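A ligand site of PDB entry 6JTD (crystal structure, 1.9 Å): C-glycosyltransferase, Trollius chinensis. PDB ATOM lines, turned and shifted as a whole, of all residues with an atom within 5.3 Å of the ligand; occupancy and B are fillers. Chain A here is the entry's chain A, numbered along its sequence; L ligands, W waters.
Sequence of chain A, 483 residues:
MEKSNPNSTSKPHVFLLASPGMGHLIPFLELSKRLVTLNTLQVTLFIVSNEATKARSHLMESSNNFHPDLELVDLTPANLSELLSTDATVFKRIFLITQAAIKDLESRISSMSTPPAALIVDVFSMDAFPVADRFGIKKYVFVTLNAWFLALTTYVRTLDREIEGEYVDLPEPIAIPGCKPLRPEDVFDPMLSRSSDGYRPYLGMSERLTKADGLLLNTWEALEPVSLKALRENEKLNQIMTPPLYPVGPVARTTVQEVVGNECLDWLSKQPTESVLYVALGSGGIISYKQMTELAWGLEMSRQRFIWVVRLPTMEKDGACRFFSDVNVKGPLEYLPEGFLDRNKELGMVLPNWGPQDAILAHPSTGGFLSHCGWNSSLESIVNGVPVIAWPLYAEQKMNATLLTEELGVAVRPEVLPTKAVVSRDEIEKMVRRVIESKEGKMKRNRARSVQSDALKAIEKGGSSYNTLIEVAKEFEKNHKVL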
ATOM      1  N   MET A  22       5.197   2.759  12.172  1.00  0.00           N
ATOM      2  CA  MET A  22       5.075   4.015  12.906  1.00  0.00           C
ATOM      3  C   MET A  22       6.427   4.577  13.300  1.00  0.00           C
ATOM      4  O   MET A  22       6.611   5.811  13.335  1.00  0.00           O
ATOM      5  CB  MET A  22       4.205   3.774  14.138  1.00  0.00           C
ATOM      6  CG  MET A  22       2.792   3.519  13.788  1.00  0.00           C
ATOM      7  SD  MET A  22       2.064   4.965  12.955  1.00  0.00           S
ATOM      8  CE  MET A  22       0.353   4.536  13.007  1.00  0.00           C
ATOM      9  N   GLY A  23       7.402   3.718  13.607  1.00  0.00           N
ATOM     10  CA  GLY A  23       8.722   4.159  13.965  1.00  0.00           C
ATOM     11  C   GLY A  23       9.533   4.703  12.807  1.00  0.00           C
ATOM     12  O   GLY A  23      10.609   5.241  13.027  1.00  0.00           O
ATOM     13  N   HIS A  24       9.044   4.561  11.572  1.00  0.00           N
ATOM     14  CA  HIS A  24       9.639   5.263  10.438  1.00  0.00           C
ATOM     15  C   HIS A  24       8.856   6.476  10.041  1.00  0.00           C
ATOM     16  O   HIS A  24       9.435   7.538   9.801  1.00  0.00           O
ATOM     17  CB  HIS A  24       9.764   4.302   9.251  1.00  0.00           C
ATOM     18  CG  HIS A  24      10.517   3.073   9.581  1.00  0.00           C
ATOM     19  ND1 HIS A  24      10.120   1.808   9.184  1.00  0.00           N
ATOM     20  CD2 HIS A  24      11.672   2.900  10.269  1.00  0.00           C
ATOM     21  CE1 HIS A  24      10.976   0.917   9.634  1.00  0.00           C
ATOM     22  NE2 HIS A  24      11.935   1.555  10.297  1.00  0.00           N
ATOM     23  N   ILE A  26       6.750   8.380  11.910  1.00  0.00           N
ATOM     24  CA  ILE A  26       6.685   9.481  12.868  1.00  0.00           C
ATOM     25  C   ILE A  26       7.933  10.370  12.838  1.00  0.00           C
ATOM     26  O   ILE A  26       7.784  11.596  12.726  1.00  0.00           O
ATOM     27  CB  ILE A  26       6.340   8.925  14.256  1.00  0.00           C
ATOM     28  CG1 ILE A  26       4.872   8.557  14.341  1.00  0.00           C
ATOM     29  CG2 ILE A  26       6.744   9.923  15.366  1.00  0.00           C
ATOM     30  CD1 ILE A  26       4.469   7.760  15.532  1.00  0.00           C
ATOM     31  N   ARG A 253       8.599  14.193  18.675  1.00  0.00           N
ATOM     32  CA  ARG A 253       7.518  15.145  18.954  1.00  0.00           C
ATOM     33  C   ARG A 253       7.839  15.902  20.250  1.00  0.00           C
ATOM     34  O   ARG A 253       7.805  15.329  21.344  1.00  0.00           O
ATOM     35  CB  ARG A 253       6.193  14.405  19.012  1.00  0.00           C
ATOM     36  CG  ARG A 253       5.804  13.780  17.651  1.00  0.00           C
ATOM     37  CD  ARG A 253       4.551  12.937  17.679  1.00  0.00           C
ATOM     38  NE  ARG A 253       4.773  11.659  18.343  1.00  0.00           N
ATOM     39  CZ  ARG A 253       3.858  10.718  18.521  1.00  0.00           C
ATOM     40  NH1 ARG A 253       4.189   9.616  19.169  1.00  0.00           N
ATOM     41  NH2 ARG A 253       2.628  10.853  18.048  1.00  0.00           N
ATOM     42  N   TYR A 278       3.040   4.920  32.291  1.00  0.00           N
ATOM     43  CA  TYR A 278       2.616   4.588  30.945  1.00  0.00           C
ATOM     44  C   TYR A 278       3.310   3.297  30.501  1.00  0.00           C
ATOM     45  O   TYR A 278       4.522   3.165  30.630  1.00  0.00           O
ATOM     46  CB  TYR A 278       2.930   5.745  29.996  1.00  0.00           C
ATOM     47  CG  TYR A 278       2.622   5.466  28.543  1.00  0.00           C
ATOM     48  CD1 TYR A 278       1.332   5.221  28.125  1.00  0.00           C
ATOM     49  CD2 TYR A 278       3.615   5.503  27.591  1.00  0.00           C
ATOM     50  CE1 TYR A 278       1.037   4.980  26.785  1.00  0.00           C
ATOM     51  CE2 TYR A 278       3.350   5.306  26.238  1.00  0.00           C
ATOM     52  CZ  TYR A 278       2.056   5.032  25.834  1.00  0.00           C
ATOM     53  OH  TYR A 278       1.788   4.819  24.509  1.00  0.00           O
ATOM     54  N   ALA A 280       3.641   0.736  27.286  1.00  0.00           N
ATOM     55  CA  ALA A 280       3.320   0.524  25.880  1.00  0.00           C
ATOM     56  C   ALA A 280       4.584   0.028  25.213  1.00  0.00           C
ATOM     57  O   ALA A 280       5.630   0.689  25.305  1.00  0.00           O
ATOM     58  CB  ALA A 280       2.816   1.811  25.216  1.00  0.00           C
ATOM     59  N   LEU A 281       4.488  -1.127  24.555  1.00  0.00           N
ATOM     60  CA  LEU A 281       5.658  -1.760  23.936  1.00  0.00           C
ATOM     61  C   LEU A 281       5.670  -1.425  22.448  1.00  0.00           C
ATOM     62  O   LEU A 281       5.511  -2.275  21.576  1.00  0.00           O
ATOM     63  CB  LEU A 281       5.628  -3.260  24.185  1.00  0.00           C
ATOM     64  CG  LEU A 281       5.540  -3.667  25.659  1.00  0.00           C
ATOM     65  CD1 LEU A 281       5.432  -5.168  25.871  1.00  0.00           C
ATOM     66  CD2 LEU A 281       6.767  -3.120  26.386  1.00  0.00           C
ATOM     67  N   GLY A 282       5.787  -0.131  22.183  1.00  0.00           N
ATOM     68  CA  GLY A 282       5.856   0.397  20.842  1.00  0.00           C
ATOM     69  C   GLY A 282       4.589   0.205  20.032  1.00  0.00           C
ATOM     70  O   GLY A 282       3.492  -0.055  20.552  1.00  0.00           O
ATOM     71  N   SER A 283       4.759   0.373  18.710  1.00  0.00           N
ATOM     72  CA  SER A 283       3.690   0.052  17.782  1.00  0.00           C
ATOM     73  C   SER A 283       3.714  -1.432  17.414  1.00  0.00           C
ATOM     74  O   SER A 283       2.685  -1.986  17.016  1.00  0.00           O
ATOM     75  CB  SER A 283       3.786   0.950  16.561  1.00  0.00           C
ATOM     76  OG  SER A 283       4.856   0.597  15.711  1.00  0.00           O
ATOM     77  N   GLY A 284       4.878  -2.089  17.500  1.00  0.00           N
ATOM     78  CA  GLY A 284       5.014  -3.431  16.955  1.00  0.00           C
ATOM     79  C   GLY A 284       5.186  -4.536  17.992  1.00  0.00           C
ATOM     80  O   GLY A 284       5.274  -5.721  17.645  1.00  0.00           O
ATOM     81  N   GLY A 285       5.262  -4.160  19.266  1.00  0.00           N
ATOM     82  CA  GLY A 285       5.584  -5.119  20.300  1.00  0.00           C
ATOM     83  C   GLY A 285       4.369  -5.950  20.699  1.00  0.00           C
ATOM     84  O   GLY A 285       3.268  -5.424  20.883  1.00  0.00           O
ATOM     85  N   VAL A 309      -1.258   0.171  27.051  1.00  0.00           N
ATOM     86  CA  VAL A 309      -1.653  -0.108  25.669  1.00  0.00           C
ATOM     87  C   VAL A 309      -1.479  -1.613  25.439  1.00  0.00           C
ATOM     88  O   VAL A 309      -0.366  -2.151  25.538  1.00  0.00           O
ATOM     89  CB  VAL A 309      -0.790   0.690  24.669  1.00  0.00           C
ATOM     90  CG1 VAL A 309      -1.185   0.353  23.258  1.00  0.00           C
ATOM     91  CG2 VAL A 309      -0.971   2.182  24.911  1.00  0.00           C
ATOM     92  N   ARG A 311      -2.313  -5.222  23.097  1.00  0.00           N
ATOM     93  CA  ARG A 311      -2.694  -5.836  21.834  1.00  0.00           C
ATOM     94  C   ARG A 311      -2.999  -7.317  22.033  1.00  0.00           C
ATOM     95  O   ARG A 311      -2.739  -7.893  23.094  1.00  0.00           O
ATOM     96  CB  ARG A 311      -1.623  -5.723  20.742  1.00  0.00           C
ATOM     97  CG  ARG A 311      -0.579  -4.724  20.902  1.00  0.00           C
ATOM     98  CD  ARG A 311       0.161  -4.455  19.550  1.00  0.00           C
ATOM     99  NE  ARG A 311       0.140  -3.010  19.450  1.00  0.00           N
ATOM    100  CZ  ARG A 311       1.084  -2.219  19.930  1.00  0.00           C
ATOM    101  NH1 ARG A 311       2.202  -2.725  20.464  1.00  0.00           N
ATOM    102  NH2 ARG A 311       0.910  -0.906  19.860  1.00  0.00           N
ATOM    103  N   ASN A 353      -4.426  -1.378  21.492  1.00  0.00           N
ATOM    104  CA  ASN A 353      -3.647  -1.056  20.255  1.00  0.00           C
ATOM    105  C   ASN A 353      -2.830   0.240  20.227  1.00  0.00           C
ATOM    106  O   ASN A 353      -1.636   0.197  19.960  1.00  0.00           O
ATOM    107  CB  ASN A 353      -4.588  -1.084  19.050  1.00  0.00           C
ATOM    108  CG  ASN A 353      -5.244  -2.422  18.852  1.00  0.00           C
ATOM    109  OD1 ASN A 353      -4.566  -3.444  18.745  1.00  0.00           O
ATOM    110  ND2 ASN A 353      -6.565  -2.450  18.834  1.00  0.00           N
ATOM    111  N   TRP A 354      -3.456   1.401  20.435  1.00  0.00           N
ATOM    112  CA  TRP A 354      -2.793   2.675  20.269  1.00  0.00           C
ATOM    113  C   TRP A 354      -3.180   3.644  21.386  1.00  0.00           C
ATOM    114  O   TRP A 354      -4.350   3.772  21.711  1.00  0.00           O
ATOM    115  CB  TRP A 354      -3.234   3.256  18.934  1.00  0.00           C
ATOM    116  CG  TRP A 354      -2.483   4.436  18.470  1.00  0.00           C
ATOM    117  CD1 TRP A 354      -2.939   5.718  18.424  1.00  0.00           C
ATOM    118  CD2 TRP A 354      -1.159   4.453  17.938  1.00  0.00           C
ATOM    119  NE1 TRP A 354      -1.970   6.541  17.917  1.00  0.00           N
ATOM    120  CE2 TRP A 354      -0.862   5.792  17.599  1.00  0.00           C
ATOM    121  CE3 TRP A 354      -0.187   3.481  17.708  1.00  0.00           C
ATOM    122  CZ2 TRP A 354       0.359   6.171  17.060  1.00  0.00           C
ATOM    123  CZ3 TRP A 354       1.020   3.856  17.174  1.00  0.00           C
ATOM    124  CH2 TRP A 354       1.287   5.195  16.863  1.00  0.00           C
ATOM    125  N   GLY A 355      -2.204   4.344  21.951  1.00  0.00           N
ATOM    126  CA  GLY A 355      -2.491   5.440  22.838  1.00  0.00           C
ATOM    127  C   GLY A 355      -1.841   6.712  22.373  1.00  0.00           C
ATOM    128  O   GLY A 355      -0.922   6.697  21.541  1.00  0.00           O
ATOM    129  N   PRO A 356      -2.268   7.863  22.940  1.00  0.00           N
ATOM    130  CA  PRO A 356      -1.664   9.152  22.543  1.00  0.00           C
ATOM    131  C   PRO A 356      -0.342   9.363  23.265  1.00  0.00           C
ATOM    132  O   PRO A 356      -0.212  10.216  24.202  1.00  0.00           O
ATOM    133  CB  PRO A 356      -2.750  10.156  22.938  1.00  0.00           C
ATOM    134  CG  PRO A 356      -3.433   9.524  24.119  1.00  0.00           C
ATOM    135  CD  PRO A 356      -3.389   8.023  23.889  1.00  0.00           C
ATOM    136  N   GLN A 357       0.656   8.623  22.805  1.00  0.00           N
ATOM    137  CA  GLN A 357       1.921   8.530  23.551  1.00  0.00           C
ATOM    138  C   GLN A 357       2.628   9.878  23.698  1.00  0.00           C
ATOM    139  O   GLN A 357       3.197  10.170  24.762  1.00  0.00           O
ATOM    140  CB  GLN A 357       2.845   7.544  22.830  1.00  0.00           C
ATOM    141  CG  GLN A 357       4.181   7.350  23.437  1.00  0.00           C
ATOM    142  CD  GLN A 357       4.813   6.010  23.109  1.00  0.00           C
ATOM    143  OE1 GLN A 357       4.127   4.977  23.037  1.00  0.00           O
ATOM    144  NE2 GLN A 357       6.130   6.017  22.928  1.00  0.00           N
ATOM    145  N   ASP A 358       2.647  10.698  22.646  1.00  0.00           N
ATOM    146  CA  ASP A 358       3.335  11.988  22.752  1.00  0.00           C
ATOM    147  C   ASP A 358       2.724  12.830  23.844  1.00  0.00           C
ATOM    148  O   ASP A 358       3.444  13.437  24.652  1.00  0.00           O
ATOM    149  CB  ASP A 358       3.298  12.752  21.413  1.00  0.00           C
ATOM    150  CG  ASP A 358       1.888  12.980  20.872  1.00  0.00           C
ATOM    151  OD1 ASP A 358       0.885  12.318  21.271  1.00  0.00           O
ATOM    152  OD2 ASP A 358       1.796  13.811  19.951  1.00  0.00           O
ATOM    153  N   HIS A 372       9.397  -0.649  25.294  1.00  0.00           N
ATOM    154  CA  HIS A 372      10.221  -1.652  24.633  1.00  0.00           C
ATOM    155  C   HIS A 372      11.520  -1.048  24.129  1.00  0.00           C
ATOM    156  O   HIS A 372      12.362  -1.782  23.572  1.00  0.00           O
ATOM    157  CB  HIS A 372       9.448  -2.343  23.494  1.00  0.00           C
ATOM    158  CG  HIS A 372       9.267  -1.533  22.253  1.00  0.00           C
ATOM    159  ND1 HIS A 372       9.406  -0.151  22.207  1.00  0.00           N
ATOM    160  CD2 HIS A 372       8.910  -1.902  21.009  1.00  0.00           C
ATOM    161  CE1 HIS A 372       9.186   0.269  20.975  1.00  0.00           C
ATOM    162  NE2 HIS A 372       8.874  -0.757  20.231  1.00  0.00           N
ATOM    163  N   GLY A 374      12.248   0.901  21.720  1.00  0.00           N
ATOM    164  CA  GLY A 374      12.447   1.375  20.357  1.00  0.00           C
ATOM    165  C   GLY A 374      12.982   2.794  20.387  1.00  0.00           C
ATOM    166  O   GLY A 374      12.771   3.523  21.368  1.00  0.00           O
ATOM    167  N   TRP A 375      13.687   3.209  19.325  1.00  0.00           N
ATOM    168  CA  TRP A 375      14.459   4.444  19.492  1.00  0.00           C
ATOM    169  C   TRP A 375      13.518   5.658  19.564  1.00  0.00           C
ATOM    170  O   TRP A 375      13.789   6.626  20.268  1.00  0.00           O
ATOM    171  CB  TRP A 375      15.516   4.607  18.395  1.00  0.00           C
ATOM    172  CG  TRP A 375      16.513   5.733  18.753  1.00  0.00           C
ATOM    173  CD1 TRP A 375      16.831   6.844  17.997  1.00  0.00           C
ATOM    174  CD2 TRP A 375      17.270   5.841  19.969  1.00  0.00           C
ATOM    175  NE1 TRP A 375      17.749   7.641  18.690  1.00  0.00           N
ATOM    176  CE2 TRP A 375      18.019   7.058  19.894  1.00  0.00           C
ATOM    177  CE3 TRP A 375      17.385   5.045  21.117  1.00  0.00           C
ATOM    178  CZ2 TRP A 375      18.863   7.481  20.925  1.00  0.00           C
ATOM    179  CZ3 TRP A 375      18.241   5.464  22.137  1.00  0.00           C
ATOM    180  CH2 TRP A 375      18.949   6.667  22.035  1.00  0.00           C
ATOM    181  N   ASN A 376      12.411   5.663  18.813  1.00  0.00           N
ATOM    182  CA  ASN A 376      11.508   6.818  18.912  1.00  0.00           C
ATOM    183  C   ASN A 376      10.939   6.936  20.321  1.00  0.00           C
ATOM    184  O   ASN A 376      10.876   8.036  20.898  1.00  0.00           O
ATOM    185  CB  ASN A 376      10.400   6.747  17.888  1.00  0.00           C
ATOM    186  CG  ASN A 376      10.912   6.862  16.496  1.00  0.00           C
ATOM    187  OD1 ASN A 376      11.362   7.918  16.087  1.00  0.00           O
ATOM    188  ND2 ASN A 376      10.875   5.754  15.766  1.00  0.00           N
ATOM    189  N   SER A 377      10.506   5.809  20.890  1.00  0.00           N
ATOM    190  CA  SER A 377       9.935   5.829  22.227  1.00  0.00           C
ATOM    191  C   SER A 377      10.975   6.265  23.240  1.00  0.00           C
ATOM    192  O   SER A 377      10.681   7.018  24.160  1.00  0.00           O
ATOM    193  CB  SER A 377       9.381   4.444  22.603  1.00  0.00           C
ATOM    194  OG  SER A 377       8.248   4.079  21.842  1.00  0.00           O
ATOM    195  N   SER A 378      12.219   5.781  23.067  1.00  0.00           N
ATOM    196  CA  SER A 378      13.315   6.195  23.935  1.00  0.00           C
ATOM    197  C   SER A 378      13.493   7.705  23.905  1.00  0.00           C
ATOM    198  O   SER A 378      13.653   8.354  24.949  1.00  0.00           O
ATOM    199  CB  SER A 378      14.619   5.511  23.510  1.00  0.00           C
ATOM    200  OG  SER A 378      14.556   4.098  23.637  1.00  0.00           O
ATOM    201  N   GLU A 380      11.322   9.934  22.999  1.00  0.00           N
ATOM    202  CA  GLU A 380      10.173  10.607  23.594  1.00  0.00           C
ATOM    203  C   GLU A 380      10.266  10.578  25.122  1.00  0.00           C
ATOM    204  O   GLU A 380       9.850  11.555  25.783  1.00  0.00           O
ATOM    205  CB  GLU A 380       8.865   9.978  23.125  1.00  0.00           C
ATOM    206  CG  GLU A 380       8.645  10.202  21.624  1.00  0.00           C
ATOM    207  CD  GLU A 380       7.608   9.264  21.023  1.00  0.00           C
ATOM    208  OE1 GLU A 380       7.136   8.306  21.697  1.00  0.00           O
ATOM    209  OE2 GLU A 380       7.245   9.503  19.842  1.00  0.00           O
ATOM    210  N   TYR A 394      12.684  -6.441  20.165  1.00  0.00           N
ATOM    211  CA  TYR A 394      13.083  -6.761  18.797  1.00  0.00           C
ATOM    212  C   TYR A 394      13.930  -5.614  18.266  1.00  0.00           C
ATOM    213  O   TYR A 394      14.278  -4.688  18.992  1.00  0.00           O
ATOM    214  CB  TYR A 394      11.859  -7.064  17.899  1.00  0.00           C
ATOM    215  CG  TYR A 394      10.862  -5.954  17.810  1.00  0.00           C
ATOM    216  CD1 TYR A 394       9.852  -5.819  18.724  1.00  0.00           C
ATOM    217  CD2 TYR A 394      10.930  -5.002  16.785  1.00  0.00           C
ATOM    218  CE1 TYR A 394       8.916  -4.775  18.654  1.00  0.00           C
ATOM    219  CE2 TYR A 394       9.998  -3.958  16.701  1.00  0.00           C
ATOM    220  CZ  TYR A 394       8.998  -3.859  17.649  1.00  0.00           C
ATOM    221  OH  TYR A 394       8.060  -2.834  17.637  1.00  0.00           O
ATOM    222  N   GLN A 397      16.433  -2.903  20.070  1.00  0.00           N
ATOM    223  CA  GLN A 397      15.921  -2.450  21.344  1.00  0.00           C
ATOM    224  C   GLN A 397      16.797  -2.897  22.514  1.00  0.00           C
ATOM    225  O   GLN A 397      16.921  -2.163  23.481  1.00  0.00           O
ATOM    226  CB  GLN A 397      14.491  -2.928  21.544  1.00  0.00           C
ATOM    227  CG  GLN A 397      13.496  -2.164  20.629  1.00  0.00           C
ATOM    228  CD  GLN A 397      12.268  -2.953  20.332  1.00  0.00           C
ATOM    229  OE1 GLN A 397      11.905  -3.875  21.051  1.00  0.00           O
ATOM    230  NE2 GLN A 397      11.633  -2.631  19.204  1.00  0.00           N
HETATM  231  N1  LIG L   1       3.223   5.191  19.435  1.00  0.00           N
HETATM  232  C1  LIG L   1       2.127   5.814  19.788  1.00  0.00           C
HETATM  233  N2  LIG L   1       1.171   5.185  20.442  1.00  0.00           N
HETATM  234  C2  LIG L   1       1.290   3.913  20.789  1.00  0.00           C
HETATM  235  C3  LIG L   1       2.445   3.187  20.447  1.00  0.00           C
HETATM  236  C4  LIG L   1       3.416   3.899  19.730  1.00  0.00           C
HETATM  237  O1  LIG L   1       1.978   6.977  19.529  1.00  0.00           O
HETATM  238  O2  LIG L   1       0.254   3.313  21.487  1.00  0.00           O
HETATM  239  C5  LIG L   1       4.267   5.898  18.760  1.00  0.00           C
HETATM  240  C6  LIG L   1       5.337   6.050  19.558  1.00  0.00           C
HETATM  241  O3  LIG L   1       5.153   7.325  20.303  1.00  0.00           O
HETATM  242  C7  LIG L   1       6.593   6.173  18.710  1.00  0.00           C
HETATM  243  C8  LIG L   1       6.168   5.108  17.595  1.00  0.00           C
HETATM  244  O4  LIG L   1       4.882   4.996  17.655  1.00  0.00           O
HETATM  245  O5  LIG L   1       6.857   7.352  18.070  1.00  0.00           O
HETATM  246  C9  LIG L   1       6.879   3.720  17.842  1.00  0.00           C
HETATM  247  O6  LIG L   1       8.191   3.892  17.385  1.00  0.00           O
HETATM  248  P1  LIG L   1       9.421   3.096  18.132  1.00  0.00           P
HETATM  249  O7  LIG L   1      10.699   3.560  17.499  1.00  0.00           O
HETATM  250  O8  LIG L   1       9.454   3.335  19.617  1.00  0.00           O
HETATM  251  O9  LIG L   1       9.211   1.513  17.999  1.00  0.00           O
HETATM  252  P2  LIG L   1       8.467   0.570  16.916  1.00  0.00           P
HETATM  253  O10 LIG L   1       9.277  -0.708  16.881  1.00  0.00           O
HETATM  254  O11 LIG L   1       8.497   1.225  15.555  1.00  0.00           O
HETATM  255  O12 LIG L   1       7.176   0.298  17.521  1.00  0.00           O
HETATM  256  O   HOH W   1      12.139  -0.630  17.054  1.00  0.00           O
HETATM  257  O   HOH W   2      11.171   1.026  13.941  1.00  0.00           O
HETATM  258  O   HOH W   3      12.488   2.939  15.976  1.00  0.00           O
HETATM  259  O   HOH W   4       0.623   9.343  19.334  1.00  0.00           O
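Merely in contact with the ligand: Met 22, Ile 26, Tyr 278, Gly 282, Val 309, Asn 353, Trp 354, Gly 374, Trp 375 and Gln 397.
Hydrophobic or aromatic side chains that line the ligand: Met 22, Ile 26, Val 309, Trp 354, His 372 and Tyr 394.
Within 4 Å of the ligand: Met 22, Gly 23, Ile 26, Arg 253, Tyr 278, Gly 282, Ser 283, Gly 284, Val 309, Asn 353, Trp 354, Gly 355, Gln 357, His 372, Gly 374, Trp 375, Asn 376, Ser 377, Glu 380, Tyr 394 and Gln 397.
Water W3 lies within hydrogen-bond range of an oxygen (O7) of the ligand and the side-chain amide nitrogen (ND2) of Asn 376.
Water W4 bridges O1 of the ligand (2.7 Å) and NH2 of Arg 253 (2.8 Å).
Water W1 bridges O10 of the ligand (2.9 Å) and NE2 of Gln 397 (3.0 Å).
O of Asn 353 lies within hydrogen-bond range of NH2 of Arg 311, 2.8 Å away.
The backbone NH of Gly 374 lies within hydrogen-bond range of a ring nitrogen (ND1) of His 372.
The side-chain carboxylate (OE1) of Glu 380 sits at hydrogen-bond distance from the side-chain amide nitrogen (NE2) of Gln 357 (2.8 Å).
The side-chain amide nitrogen (ND2) of Asn 376 lies within hydrogen-bond range of the backbone carbonyl oxygen (O) of Gly 23 (2.8 Å).
OE2 of Glu 380 is in salt-bridge range of NH1 of Arg 253, at 3.1 Å.
The guanidinium group of Arg 253 lies within salt-bridge range of the side-chain carboxylate of Asp 358 (3.6 Å).
The side-chain hydroxyl of Ser 378 lies within hydrogen-bond range of the backbone carbonyl oxygen of Gly 374 (2.9 Å).
OG of Ser 377 sits at hydrogen-bond distance from NE2 of Gln 357, 3.1 Å away.
O9 of the ligand is in hydrogen-bond range of NE2 of His 372, 3.2 Å away.
The side-chain hydroxyl (OG) of Ser 377 is in hydrogen-bond range of an oxygen (O8) of the ligand (2.6 Å).
The side-chain amide nitrogen (ND2) of Asn 376 sits at hydrogen-bond distance from an oxygen (O7) of the ligand, 2.8 Å away.
The backbone NH (N) of Gly 23 lies close to an oxygen (O11) of the ligand, at 3.3 Å.
N2 of the ligand is in hydrogen-bond range of O of Gly 355 (2.8 Å).
An oxygen (O3) of the ligand sits at hydrogen-bond distance from the guanidinium group (NH1) of Arg 253 (2.7 Å).
The backbone NH (N) of Asn 376 lies within hydrogen-bond range of an oxygen (O7) of the ligand.
OG of Ser 283 sits at hydrogen-bond distance from O12 of the ligand (3.0 Å).
O3 of the ligand is in hydrogen-bond range of NE2 of Gln 357, 3.1 Å away.
O10 of the ligand lies within hydrogen-bond range of OH of Tyr 394.
O12 of the ligand sits at hydrogen-bond distance from N of Gly 284 (3.3 Å).
An oxygen (O8) of the ligand lies within hydrogen-bond range of the backbone NH (N) of Ser 377.
The backbone NH (N) of Gly 355 is in hydrogen-bond range of an oxygen (O2) of the ligand.
An oxygen (O12) of the ligand is in hydrogen-bond range of the backbone NH (N) of Ser 283 (2.7 Å).
An oxygen (O3) of the ligand lies within hydrogen-bond range of the side-chain carboxylate (OE1) of Glu 380, 2.6 Å away.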
